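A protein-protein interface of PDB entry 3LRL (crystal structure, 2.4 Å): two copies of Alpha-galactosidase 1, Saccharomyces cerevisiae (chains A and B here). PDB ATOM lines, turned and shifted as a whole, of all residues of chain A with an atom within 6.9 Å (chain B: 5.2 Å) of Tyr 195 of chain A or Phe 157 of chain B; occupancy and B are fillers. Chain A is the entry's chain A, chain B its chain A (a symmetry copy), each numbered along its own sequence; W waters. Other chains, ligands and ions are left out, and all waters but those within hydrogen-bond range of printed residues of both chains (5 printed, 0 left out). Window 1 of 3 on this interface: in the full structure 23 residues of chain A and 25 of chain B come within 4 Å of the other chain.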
ATOM      1  N   THR A 159     -22.531  -9.448 -26.694  1.00  0.00           N
ATOM      2  CA  THR A 159     -21.300  -8.822 -27.155  1.00  0.00           C
ATOM      3  C   THR A 159     -21.742  -7.555 -27.897  1.00  0.00           C
ATOM      4  O   THR A 159     -22.883  -7.508 -28.394  1.00  0.00           O
ATOM      5  CB  THR A 159     -20.529  -9.722 -28.159  1.00  0.00           C
ATOM      6  OG1 THR A 159     -21.291  -9.860 -29.368  1.00  0.00           O
ATOM      7  CG2 THR A 159     -20.247 -11.092 -27.580  1.00  0.00           C
ATOM      8  N   PRO A 160     -20.881  -6.512 -27.951  1.00  0.00           N
ATOM      9  CA  PRO A 160     -21.197  -5.285 -28.718  1.00  0.00           C
ATOM     10  C   PRO A 160     -21.619  -5.535 -30.172  1.00  0.00           C
ATOM     11  O   PRO A 160     -22.601  -4.974 -30.639  1.00  0.00           O
ATOM     12  CB  PRO A 160     -19.882  -4.488 -28.646  1.00  0.00           C
ATOM     13  CG  PRO A 160     -19.312  -4.892 -27.294  1.00  0.00           C
ATOM     14  CD  PRO A 160     -19.604  -6.372 -27.213  1.00  0.00           C
ATOM     15  N   GLU A 161     -20.869  -6.377 -30.868  1.00  0.00           N
ATOM     16  CA  GLU A 161     -21.115  -6.668 -32.258  1.00  0.00           C
ATOM     17  C   GLU A 161     -22.524  -7.196 -32.564  1.00  0.00           C
ATOM     18  O   GLU A 161     -23.174  -6.687 -33.472  1.00  0.00           O
ATOM     19  CB  GLU A 161     -20.069  -7.656 -32.774  1.00  0.00           C
ATOM     20  CG  GLU A 161     -20.013  -7.698 -34.281  1.00  0.00           C
ATOM     21  CD  GLU A 161     -19.520  -9.031 -34.826  1.00  0.00           C
ATOM     22  OE1 GLU A 161     -18.854  -9.010 -35.892  1.00  0.00           O
ATOM     23  OE2 GLU A 161     -19.807 -10.091 -34.207  1.00  0.00           O
ATOM     24  N   ASP A 191     -24.317  -4.416 -23.612  1.00  0.00           N
ATOM     25  CA  ASP A 191     -23.158  -4.523 -24.512  1.00  0.00           C
ATOM     26  C   ASP A 191     -22.553  -3.168 -24.909  1.00  0.00           C
ATOM     27  O   ASP A 191     -22.128  -2.985 -26.047  1.00  0.00           O
ATOM     28  CB  ASP A 191     -23.476  -5.380 -25.752  1.00  0.00           C
ATOM     29  CG  ASP A 191     -24.048  -6.725 -25.380  1.00  0.00           C
ATOM     30  OD1 ASP A 191     -23.478  -7.345 -24.468  1.00  0.00           O
ATOM     31  OD2 ASP A 191     -25.064  -7.162 -25.973  1.00  0.00           O
ATOM     32  N   LEU A 192     -22.509  -2.245 -23.943  1.00  0.00           N
ATOM     33  CA  LEU A 192     -21.735  -0.999 -24.014  1.00  0.00           C
ATOM     34  C   LEU A 192     -22.273  -0.078 -25.097  1.00  0.00           C
ATOM     35  O   LEU A 192     -21.534   0.375 -25.956  1.00  0.00           O
ATOM     36  CB  LEU A 192     -20.226  -1.281 -24.180  1.00  0.00           C
ATOM     37  CG  LEU A 192     -19.515  -2.132 -23.114  1.00  0.00           C
ATOM     38  CD1 LEU A 192     -18.302  -2.951 -23.633  1.00  0.00           C
ATOM     39  CD2 LEU A 192     -19.100  -1.247 -21.974  1.00  0.00           C
ATOM     40  N   THR A 193     -23.566   0.227 -25.028  1.00  0.00           N
ATOM     41  CA  THR A 193     -24.239   0.953 -26.096  1.00  0.00           C
ATOM     42  C   THR A 193     -23.651   2.337 -26.392  1.00  0.00           C
ATOM     43  O   THR A 193     -23.670   2.789 -27.546  1.00  0.00           O
ATOM     44  CB  THR A 193     -25.724   1.076 -25.813  1.00  0.00           C
ATOM     45  OG1 THR A 193     -26.195  -0.175 -25.293  1.00  0.00           O
ATOM     46  CG2 THR A 193     -26.478   1.431 -27.096  1.00  0.00           C
ATOM     47  N   PHE A 194     -23.118   2.994 -25.367  1.00  0.00           N
ATOM     48  CA  PHE A 194     -22.537   4.315 -25.535  1.00  0.00           C
ATOM     49  C   PHE A 194     -21.451   4.307 -26.629  1.00  0.00           C
ATOM     50  O   PHE A 194     -21.221   5.330 -27.297  1.00  0.00           O
ATOM     51  CB  PHE A 194     -21.980   4.856 -24.201  1.00  0.00           C
ATOM     52  CG  PHE A 194     -20.915   3.985 -23.587  1.00  0.00           C
ATOM     53  CD1 PHE A 194     -19.599   4.098 -23.979  1.00  0.00           C
ATOM     54  CD2 PHE A 194     -21.243   3.043 -22.626  1.00  0.00           C
ATOM     55  CE1 PHE A 194     -18.627   3.281 -23.431  1.00  0.00           C
ATOM     56  CE2 PHE A 194     -20.283   2.231 -22.069  1.00  0.00           C
ATOM     57  CZ  PHE A 194     -18.962   2.349 -22.461  1.00  0.00           C
ATOM     58  N   TYR A 195     -20.801   3.155 -26.821  1.00  0.00           N
ATOM     59  CA  TYR A 195     -19.717   3.055 -27.787  1.00  0.00           C
ATOM     60  C   TYR A 195     -20.185   3.033 -29.248  1.00  0.00           C
ATOM     61  O   TYR A 195     -19.462   3.547 -30.127  1.00  0.00           O
ATOM     62  CB  TYR A 195     -18.883   1.804 -27.527  1.00  0.00           C
ATOM     63  CG  TYR A 195     -17.660   1.993 -26.658  1.00  0.00           C
ATOM     64  CD1 TYR A 195     -17.308   1.023 -25.701  1.00  0.00           C
ATOM     65  CD2 TYR A 195     -16.840   3.132 -26.784  1.00  0.00           C
ATOM     66  CE1 TYR A 195     -16.164   1.179 -24.891  1.00  0.00           C
ATOM     67  CE2 TYR A 195     -15.689   3.297 -25.980  1.00  0.00           C
ATOM     68  CZ  TYR A 195     -15.351   2.313 -25.044  1.00  0.00           C
ATOM     69  OH  TYR A 195     -14.220   2.450 -24.253  1.00  0.00           O
ATOM     70  N   TRP A 196     -21.353   2.408 -29.506  1.00  0.00           N
ATOM     71  CA  TRP A 196     -21.783   2.134 -30.885  1.00  0.00           C
ATOM     72  C   TRP A 196     -23.085   2.768 -31.346  1.00  0.00           C
ATOM     73  O   TRP A 196     -23.420   2.698 -32.523  1.00  0.00           O
ATOM     74  CB  TRP A 196     -21.798   0.622 -31.184  1.00  0.00           C
ATOM     75  CG  TRP A 196     -22.497  -0.270 -30.159  1.00  0.00           C
ATOM     76  CD1 TRP A 196     -21.906  -0.984 -29.156  1.00  0.00           C
ATOM     77  CD2 TRP A 196     -23.905  -0.567 -30.081  1.00  0.00           C
ATOM     78  NE1 TRP A 196     -22.856  -1.693 -28.444  1.00  0.00           N
ATOM     79  CE2 TRP A 196     -24.085  -1.464 -28.996  1.00  0.00           C
ATOM     80  CE3 TRP A 196     -25.028  -0.157 -30.816  1.00  0.00           C
ATOM     81  CZ2 TRP A 196     -25.339  -1.959 -28.632  1.00  0.00           C
ATOM     82  CZ3 TRP A 196     -26.269  -0.640 -30.460  1.00  0.00           C
ATOM     83  CH2 TRP A 196     -26.421  -1.546 -29.372  1.00  0.00           C
ATOM     84  N   GLY A 197     -23.806   3.399 -30.432  1.00  0.00           N
ATOM     85  CA  GLY A 197     -25.127   3.949 -30.729  1.00  0.00           C
ATOM     86  C   GLY A 197     -25.142   5.026 -31.791  1.00  0.00           C
ATOM     87  O   GLY A 197     -25.987   5.007 -32.678  1.00  0.00           O
ATOM     88  N   SER A 198     -24.191   5.959 -31.721  1.00  0.00           N
ATOM     89  CA  SER A 198     -24.251   7.203 -32.519  1.00  0.00           C
ATOM     90  C   SER A 198     -24.330   7.024 -34.034  1.00  0.00           C
ATOM     91  O   SER A 198     -24.923   7.852 -34.733  1.00  0.00           O
ATOM     92  CB  SER A 198     -23.060   8.101 -32.182  1.00  0.00           C
ATOM     93  OG  SER A 198     -21.866   7.456 -32.550  1.00  0.00           O
ATOM     94  N   GLY A 199     -23.716   5.968 -34.546  1.00  0.00           N
ATOM     95  CA  GLY A 199     -23.620   5.786 -35.990  1.00  0.00           C
ATOM     96  C   GLY A 199     -24.869   5.179 -36.582  1.00  0.00           C
ATOM     97  O   GLY A 199     -25.044   5.143 -37.801  1.00  0.00           O
ATOM     98  N   TRP A 204     -29.867   6.498 -26.877  1.00  0.00           N
ATOM     99  CA  TRP A 204     -29.850   5.124 -26.360  1.00  0.00           C
ATOM    100  C   TRP A 204     -30.052   5.090 -24.846  1.00  0.00           C
ATOM    101  O   TRP A 204     -29.329   5.735 -24.088  1.00  0.00           O
ATOM    102  CB  TRP A 204     -28.543   4.384 -26.734  1.00  0.00           C
ATOM    103  CG  TRP A 204     -27.324   5.211 -26.523  1.00  0.00           C
ATOM    104  CD1 TRP A 204     -26.557   5.278 -25.389  1.00  0.00           C
ATOM    105  CD2 TRP A 204     -26.731   6.120 -27.462  1.00  0.00           C
ATOM    106  NE1 TRP A 204     -25.527   6.162 -25.569  1.00  0.00           N
ATOM    107  CE2 TRP A 204     -25.619   6.705 -26.828  1.00  0.00           C
ATOM    108  CE3 TRP A 204     -27.041   6.499 -28.778  1.00  0.00           C
ATOM    109  CZ2 TRP A 204     -24.803   7.651 -27.468  1.00  0.00           C
ATOM    110  CZ3 TRP A 204     -26.231   7.426 -29.419  1.00  0.00           C
ATOM    111  CH2 TRP A 204     -25.114   7.983 -28.764  1.00  0.00           C
ATOM    112  N   ASN A 252     -19.187   9.996 -24.495  1.00  0.00           N
ATOM    113  CA  ASN A 252     -19.667   9.306 -25.703  1.00  0.00           C
ATOM    114  C   ASN A 252     -21.020   9.811 -26.217  1.00  0.00           C
ATOM    115  O   ASN A 252     -21.583   9.253 -27.140  1.00  0.00           O
ATOM    116  CB  ASN A 252     -19.679   7.796 -25.507  1.00  0.00           C
ATOM    117  CG  ASN A 252     -18.306   7.180 -25.696  1.00  0.00           C
ATOM    118  OD1 ASN A 252     -17.545   7.033 -24.743  1.00  0.00           O
ATOM    119  ND2 ASN A 252     -17.983   6.822 -26.930  1.00  0.00           N
ATOM    120  N   ASN A 259     -27.014   9.848 -24.593  1.00  0.00           N
ATOM    121  CA  ASN A 259     -27.357   8.867 -23.553  1.00  0.00           C
ATOM    122  C   ASN A 259     -28.750   9.232 -23.086  1.00  0.00           C
ATOM    123  O   ASN A 259     -29.069  10.421 -22.903  1.00  0.00           O
ATOM    124  CB  ASN A 259     -26.398   8.892 -22.358  1.00  0.00           C
ATOM    125  CG  ASN A 259     -24.935   8.652 -22.751  1.00  0.00           C
ATOM    126  OD1 ASN A 259     -24.593   7.605 -23.282  1.00  0.00           O
ATOM    127  ND2 ASN A 259     -24.073   9.613 -22.452  1.00  0.00           N
ATOM    128  N   ASN B 153     -15.822   2.942 -34.081  1.00  0.00           N
ATOM    129  CA  ASN B 153     -15.389   1.685 -34.689  1.00  0.00           C
ATOM    130  C   ASN B 153     -16.525   0.783 -35.162  1.00  0.00           C
ATOM    131  O   ASN B 153     -16.291  -0.342 -35.591  1.00  0.00           O
ATOM    132  CB  ASN B 153     -14.437   0.939 -33.755  1.00  0.00           C
ATOM    133  CG  ASN B 153     -15.040   0.692 -32.385  1.00  0.00           C
ATOM    134  OD1 ASN B 153     -16.254   0.516 -32.251  1.00  0.00           O
ATOM    135  ND2 ASN B 153     -14.189   0.661 -31.362  1.00  0.00           N
ATOM    136  N   GLY B 155     -19.098  -0.883 -33.773  1.00  0.00           N
ATOM    137  CA  GLY B 155     -19.452  -2.140 -33.130  1.00  0.00           C
ATOM    138  C   GLY B 155     -18.393  -3.215 -33.229  1.00  0.00           C
ATOM    139  O   GLY B 155     -18.562  -4.286 -32.658  1.00  0.00           O
ATOM    140  N   GLN B 156     -17.295  -2.912 -33.938  1.00  0.00           N
ATOM    141  CA  GLN B 156     -16.199  -3.847 -34.194  1.00  0.00           C
ATOM    142  C   GLN B 156     -15.165  -3.913 -33.059  1.00  0.00           C
ATOM    143  O   GLN B 156     -13.966  -3.712 -33.262  1.00  0.00           O
ATOM    144  CB  GLN B 156     -15.523  -3.509 -35.529  1.00  0.00           C
ATOM    145  CG  GLN B 156     -16.373  -3.794 -36.780  1.00  0.00           C
ATOM    146  CD  GLN B 156     -15.592  -3.600 -38.081  1.00  0.00           C
ATOM    147  OE1 GLN B 156     -14.391  -3.853 -38.146  1.00  0.00           O
ATOM    148  NE2 GLN B 156     -16.281  -3.148 -39.121  1.00  0.00           N
ATOM    149  N   PHE B 157     -15.639  -4.195 -31.854  1.00  0.00           N
ATOM    150  CA  PHE B 157     -14.781  -4.346 -30.684  1.00  0.00           C
ATOM    151  C   PHE B 157     -15.567  -5.219 -29.729  1.00  0.00           C
ATOM    152  O   PHE B 157     -16.719  -5.538 -30.003  1.00  0.00           O
ATOM    153  CB  PHE B 157     -14.493  -2.976 -30.039  1.00  0.00           C
ATOM    154  CG  PHE B 157     -15.654  -2.433 -29.266  1.00  0.00           C
ATOM    155  CD1 PHE B 157     -15.773  -2.683 -27.889  1.00  0.00           C
ATOM    156  CD2 PHE B 157     -16.664  -1.711 -29.921  1.00  0.00           C
ATOM    157  CE1 PHE B 157     -16.870  -2.209 -27.176  1.00  0.00           C
ATOM    158  CE2 PHE B 157     -17.762  -1.220 -29.215  1.00  0.00           C
ATOM    159  CZ  PHE B 157     -17.866  -1.483 -27.836  1.00  0.00           C
ATOM    160  N   GLY B 158     -14.969  -5.595 -28.602  1.00  0.00           N
ATOM    161  CA  GLY B 158     -15.710  -6.334 -27.585  1.00  0.00           C
ATOM    162  C   GLY B 158     -15.106  -7.684 -27.253  1.00  0.00           C
ATOM    163  O   GLY B 158     -15.408  -8.250 -26.212  1.00  0.00           O
ATOM    164  N   THR B 159     -14.245  -8.193 -28.138  1.00  0.00           N
ATOM    165  CA  THR B 159     -13.528  -9.447 -27.951  1.00  0.00           C
ATOM    166  C   THR B 159     -12.156  -9.229 -28.598  1.00  0.00           C
ATOM    167  O   THR B 159     -12.037  -8.384 -29.503  1.00  0.00           O
ATOM    168  CB  THR B 159     -14.224 -10.629 -28.680  1.00  0.00           C
ATOM    169  OG1 THR B 159     -14.152 -10.430 -30.100  1.00  0.00           O
ATOM    170  CG2 THR B 159     -15.670 -10.774 -28.261  1.00  0.00           C
ATOM    171  N   ILE B 162     -12.126  -9.740 -32.739  1.00  0.00           N
ATOM    172  CA  ILE B 162     -12.691  -8.670 -33.568  1.00  0.00           C
ATOM    173  C   ILE B 162     -11.832  -7.386 -33.596  1.00  0.00           C
ATOM    174  O   ILE B 162     -11.692  -6.760 -34.643  1.00  0.00           O
ATOM    175  CB  ILE B 162     -14.193  -8.370 -33.228  1.00  0.00           C
ATOM    176  CG1 ILE B 162     -14.850  -7.556 -34.350  1.00  0.00           C
ATOM    177  CG2 ILE B 162     -14.342  -7.683 -31.885  1.00  0.00           C
ATOM    178  CD1 ILE B 162     -16.384  -7.458 -34.262  1.00  0.00           C
ATOM    179  N   SER B 163     -11.247  -7.005 -32.464  1.00  0.00           N
ATOM    180  CA  SER B 163     -10.346  -5.862 -32.453  1.00  0.00           C
ATOM    181  C   SER B 163      -9.046  -6.148 -33.220  1.00  0.00           C
ATOM    182  O   SER B 163      -8.615  -5.314 -34.042  1.00  0.00           O
ATOM    183  CB  SER B 163     -10.089  -5.367 -31.026  1.00  0.00           C
ATOM    184  OG  SER B 163     -11.240  -4.714 -30.518  1.00  0.00           O
ATOM    185  N   ARG B 166      -9.695  -5.944 -37.055  1.00  0.00           N
ATOM    186  CA  ARG B 166      -9.809  -4.519 -37.413  1.00  0.00           C
ATOM    187  C   ARG B 166      -8.442  -3.792 -37.511  1.00  0.00           C
ATOM    188  O   ARG B 166      -8.173  -3.082 -38.485  1.00  0.00           O
ATOM    189  CB  ARG B 166     -10.780  -3.788 -36.468  1.00  0.00           C
ATOM    190  CG  ARG B 166     -11.068  -2.309 -36.845  1.00  0.00           C
ATOM    191  CD  ARG B 166     -12.275  -1.721 -36.097  1.00  0.00           C
ATOM    192  NE  ARG B 166     -12.258  -2.051 -34.672  1.00  0.00           N
ATOM    193  CZ  ARG B 166     -11.698  -1.304 -33.727  1.00  0.00           C
ATOM    194  NH1 ARG B 166     -11.123  -0.121 -34.023  1.00  0.00           N
ATOM    195  NH2 ARG B 166     -11.735  -1.741 -32.471  1.00  0.00           N
ATOM    196  N   TRP B 188      -6.468   1.914 -26.662  1.00  0.00           N
ATOM    197  CA  TRP B 188      -6.641   2.130 -25.219  1.00  0.00           C
ATOM    198  C   TRP B 188      -6.627   0.831 -24.397  1.00  0.00           C
ATOM    199  O   TRP B 188      -7.253   0.738 -23.315  1.00  0.00           O
ATOM    200  CB  TRP B 188      -7.935   2.900 -24.957  1.00  0.00           C
ATOM    201  CG  TRP B 188      -8.239   3.987 -25.970  1.00  0.00           C
ATOM    202  CD1 TRP B 188      -7.400   4.988 -26.388  1.00  0.00           C
ATOM    203  CD2 TRP B 188      -9.487   4.204 -26.644  1.00  0.00           C
ATOM    204  NE1 TRP B 188      -8.033   5.789 -27.297  1.00  0.00           N
ATOM    205  CE2 TRP B 188      -9.318   5.334 -27.478  1.00  0.00           C
ATOM    206  CE3 TRP B 188     -10.734   3.544 -26.634  1.00  0.00           C
ATOM    207  CZ2 TRP B 188     -10.348   5.822 -28.301  1.00  0.00           C
ATOM    208  CZ3 TRP B 188     -11.754   4.026 -27.452  1.00  0.00           C
ATOM    209  CH2 TRP B 188     -11.556   5.171 -28.261  1.00  0.00           C
ATOM    210  N   GLN B 190      -8.039  -1.848 -25.235  1.00  0.00           N
ATOM    211  CA  GLN B 190      -9.324  -2.530 -25.378  1.00  0.00           C
ATOM    212  C   GLN B 190      -9.147  -3.962 -25.915  1.00  0.00           C
ATOM    213  O   GLN B 190      -8.359  -4.204 -26.852  1.00  0.00           O
ATOM    214  CB  GLN B 190     -10.272  -1.698 -26.245  1.00  0.00           C
ATOM    215  CG  GLN B 190     -11.731  -2.188 -26.392  1.00  0.00           C
ATOM    216  CD  GLN B 190     -12.561  -1.201 -27.222  1.00  0.00           C
ATOM    217  OE1 GLN B 190     -12.320  -0.991 -28.446  1.00  0.00           O
ATOM    218  NE2 GLN B 190     -13.521  -0.563 -26.563  1.00  0.00           N
ATOM    219  N   ASP B 191      -9.877  -4.895 -25.301  1.00  0.00           N
ATOM    220  CA  ASP B 191      -9.804  -6.322 -25.654  1.00  0.00           C
ATOM    221  C   ASP B 191      -8.390  -6.917 -25.549  1.00  0.00           C
ATOM    222  O   ASP B 191      -8.000  -7.742 -26.370  1.00  0.00           O
ATOM    223  CB  ASP B 191     -10.429  -6.602 -27.034  1.00  0.00           C
ATOM    224  CG  ASP B 191     -11.826  -6.048 -27.147  1.00  0.00           C
ATOM    225  OD1 ASP B 191     -12.592  -6.257 -26.191  1.00  0.00           O
ATOM    226  OD2 ASP B 191     -12.165  -5.395 -28.164  1.00  0.00           O
ATOM    227  N   LYS B 231     -13.368  -2.029 -19.482  1.00  0.00           N
ATOM    228  CA  LYS B 231     -14.433  -1.972 -20.503  1.00  0.00           C
ATOM    229  C   LYS B 231     -14.785  -0.554 -20.961  1.00  0.00           C
ATOM    230  O   LYS B 231     -15.527  -0.347 -21.917  1.00  0.00           O
ATOM    231  CB  LYS B 231     -15.691  -2.704 -20.006  1.00  0.00           C
ATOM    232  CG  LYS B 231     -15.466  -4.176 -19.637  1.00  0.00           C
ATOM    233  CD  LYS B 231     -14.981  -5.001 -20.840  1.00  0.00           C
ATOM    234  CE  LYS B 231     -14.845  -6.483 -20.478  1.00  0.00           C
ATOM    235  NZ  LYS B 231     -14.572  -7.388 -21.665  1.00  0.00           N
ATOM    236  N   TYR B 232     -14.224   0.432 -20.288  1.00  0.00           N
ATOM    237  CA  TYR B 232     -14.472   1.827 -20.621  1.00  0.00           C
ATOM    238  C   TYR B 232     -13.187   2.587 -20.331  1.00  0.00           C
ATOM    239  O   TYR B 232     -13.068   3.191 -19.263  1.00  0.00           O
ATOM    240  CB  TYR B 232     -15.619   2.403 -19.770  1.00  0.00           C
ATOM    241  CG  TYR B 232     -16.339   3.614 -20.381  1.00  0.00           C
ATOM    242  CD1 TYR B 232     -17.564   4.063 -19.848  1.00  0.00           C
ATOM    243  CD2 TYR B 232     -15.803   4.308 -21.484  1.00  0.00           C
ATOM    244  CE1 TYR B 232     -18.243   5.153 -20.398  1.00  0.00           C
ATOM    245  CE2 TYR B 232     -16.466   5.403 -22.043  1.00  0.00           C
ATOM    246  CZ  TYR B 232     -17.690   5.820 -21.492  1.00  0.00           C
ATOM    247  OH  TYR B 232     -18.363   6.894 -22.037  1.00  0.00           O
ATOM    248  N   ALA B 233     -12.238   2.535 -21.271  1.00  0.00           N
ATOM    249  CA  ALA B 233     -10.916   3.166 -21.116  1.00  0.00           C
ATOM    250  C   ALA B 233     -11.006   4.647 -20.723  1.00  0.00           C
ATOM    251  O   ALA B 233     -10.261   5.113 -19.853  1.00  0.00           O
ATOM    252  CB  ALA B 233     -10.085   3.012 -22.395  1.00  0.00           C
ATOM    253  N   GLY B 234     -11.903   5.364 -21.395  1.00  0.00           N
ATOM    254  CA  GLY B 234     -12.137   6.782 -21.128  1.00  0.00           C
ATOM    255  C   GLY B 234     -10.939   7.655 -21.385  1.00  0.00           C
ATOM    256  O   GLY B 234     -10.123   7.378 -22.275  1.00  0.00           O
HETATM  257  O   HOH W   1     -18.276  -7.794 -30.073  1.00  0.00           O
HETATM  258  O   HOH W   2     -13.139   5.064 -24.106  1.00  0.00           O
HETATM  259  O   HOH W   3     -16.647   3.459 -31.136  1.00  0.00           O
HETATM  260  O   HOH W   4     -12.418   0.313 -23.352  1.00  0.00           O
HETATM  261  O   HOH W   5     -18.618   1.132 -31.767  1.00  0.00           O
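The backbone carbonyl oxygen of Leu 192 of chain A lies within hydrogen-bond range of the indole nitrogen of Trp 196 of chain A. N of Gly 158 of chain B is in hydrogen-bond range of OD2 of Asp 191 of chain B (2.8 Å). The backbone NH of Ile 162 of chain B lies close to the side-chain hydroxyl of Thr 159 of chain B (3.4 Å).
Positions printed for both chains: 159 and 191.
OD1 of Asn 252 of chain A lies within hydrogen-bond range of OH of Tyr 232 of chain B, at 2.8 Å.
Water W5 lies within hydrogen-bond range of the side-chain amide oxygen of Asn 153 of chain B, the backbone NH of Gly 155 of chain B and the backbone carbonyl oxygen of Tyr 195 of chain A. Water W1 lies within hydrogen-bond range of O of Phe 157 of chain B (2.7 Å) and N of Glu 161 of chain A (3.1 Å). Water W2 bridges OH of Tyr 195 of chain A and N of Gly 234 of chain B. Water W4 lies within hydrogen-bond range of the side-chain hydroxyl (OH) of Tyr 195 of chain A (2.9 Å), the backbone NH (N) of Ala 233 of chain B (3.0 Å) and the backbone carbonyl oxygen (O) of Lys 231 of chain B (3.5 Å). Water W3 bridges O of Tyr 195 of chain A (3.0 Å) and N of Asn 153 of chain B (3.1 Å).
Printed residues of chain B within 4 Å of Phe 194 of chain A: Tyr 232 (3.3 Å). Tyr 195 of chain A touches just these residues of chain B: Phe 157 (3.3 Å), Gln 190 (3.6 Å), Lys 231 (3.4 Å), Tyr 232 (3.7 Å) and Ala 233 (3.6 Å). Gly 199 of chain A touches none of the printed residues of chain B. Of chain A, only Pro 160, Leu 192 and Tyr 195 come within 4 Å of Phe 157 of chain B. Printed residues of chain A within 4 Å of Ile 162 of chain B: Glu 161 (3.3 Å). The nearest residue of chain B that does not touch Tyr 195 of chain A is Trp 188 of chain B (4.3 Å). The nearest residue of chain A that does not touch Phe 157 of chain B is Trp 196 of chain A (4.2 Å). The nearest printed residue of chain A that does not touch Ile 162 of chain B is Pro 160 of chain A (6.9 Å).
Hydrophobic or aromatic side chains of chain B that line the printed part of chain A: Phe 157, Ile 162 and Tyr 232. Among the printed residues, no Asp or Glu carboxylate lies within 4 Å of a Lys or Arg side-chain nitrogen of the other chain.
Among the printed residues, merely in contact across the chains: Phe 194 of chain A with Tyr 232 of chain B (3.3 Å), Tyr 195 of chain A with Phe 157 of chain B (3.3 Å), Glu 161 of chain A with Ile 162 of chain B (3.3 Å), Tyr 195 of chain A with Lys 231 of chain B (3.4 Å), Glu 161 of chain A with Gly 155 of chain B (3.5 Å), Tyr 195 of chain A with Gln 190 of chain B (3.6 Å), Tyr 195 of chain A with Ala 233 of chain B (3.6 Å), Pro 160 of chain A with Phe 157 of chain B (3.6 Å), Leu 192 of chain A with Lys 231 of chain B (3.7 Å), Tyr 195 of chain A with Tyr 232 of chain B (3.7 Å), Pro 160 of chain A with Gly 158 of chain B (3.9 Å) and Leu 192 of chain A with Phe 157 of chain B (3.9 Å).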
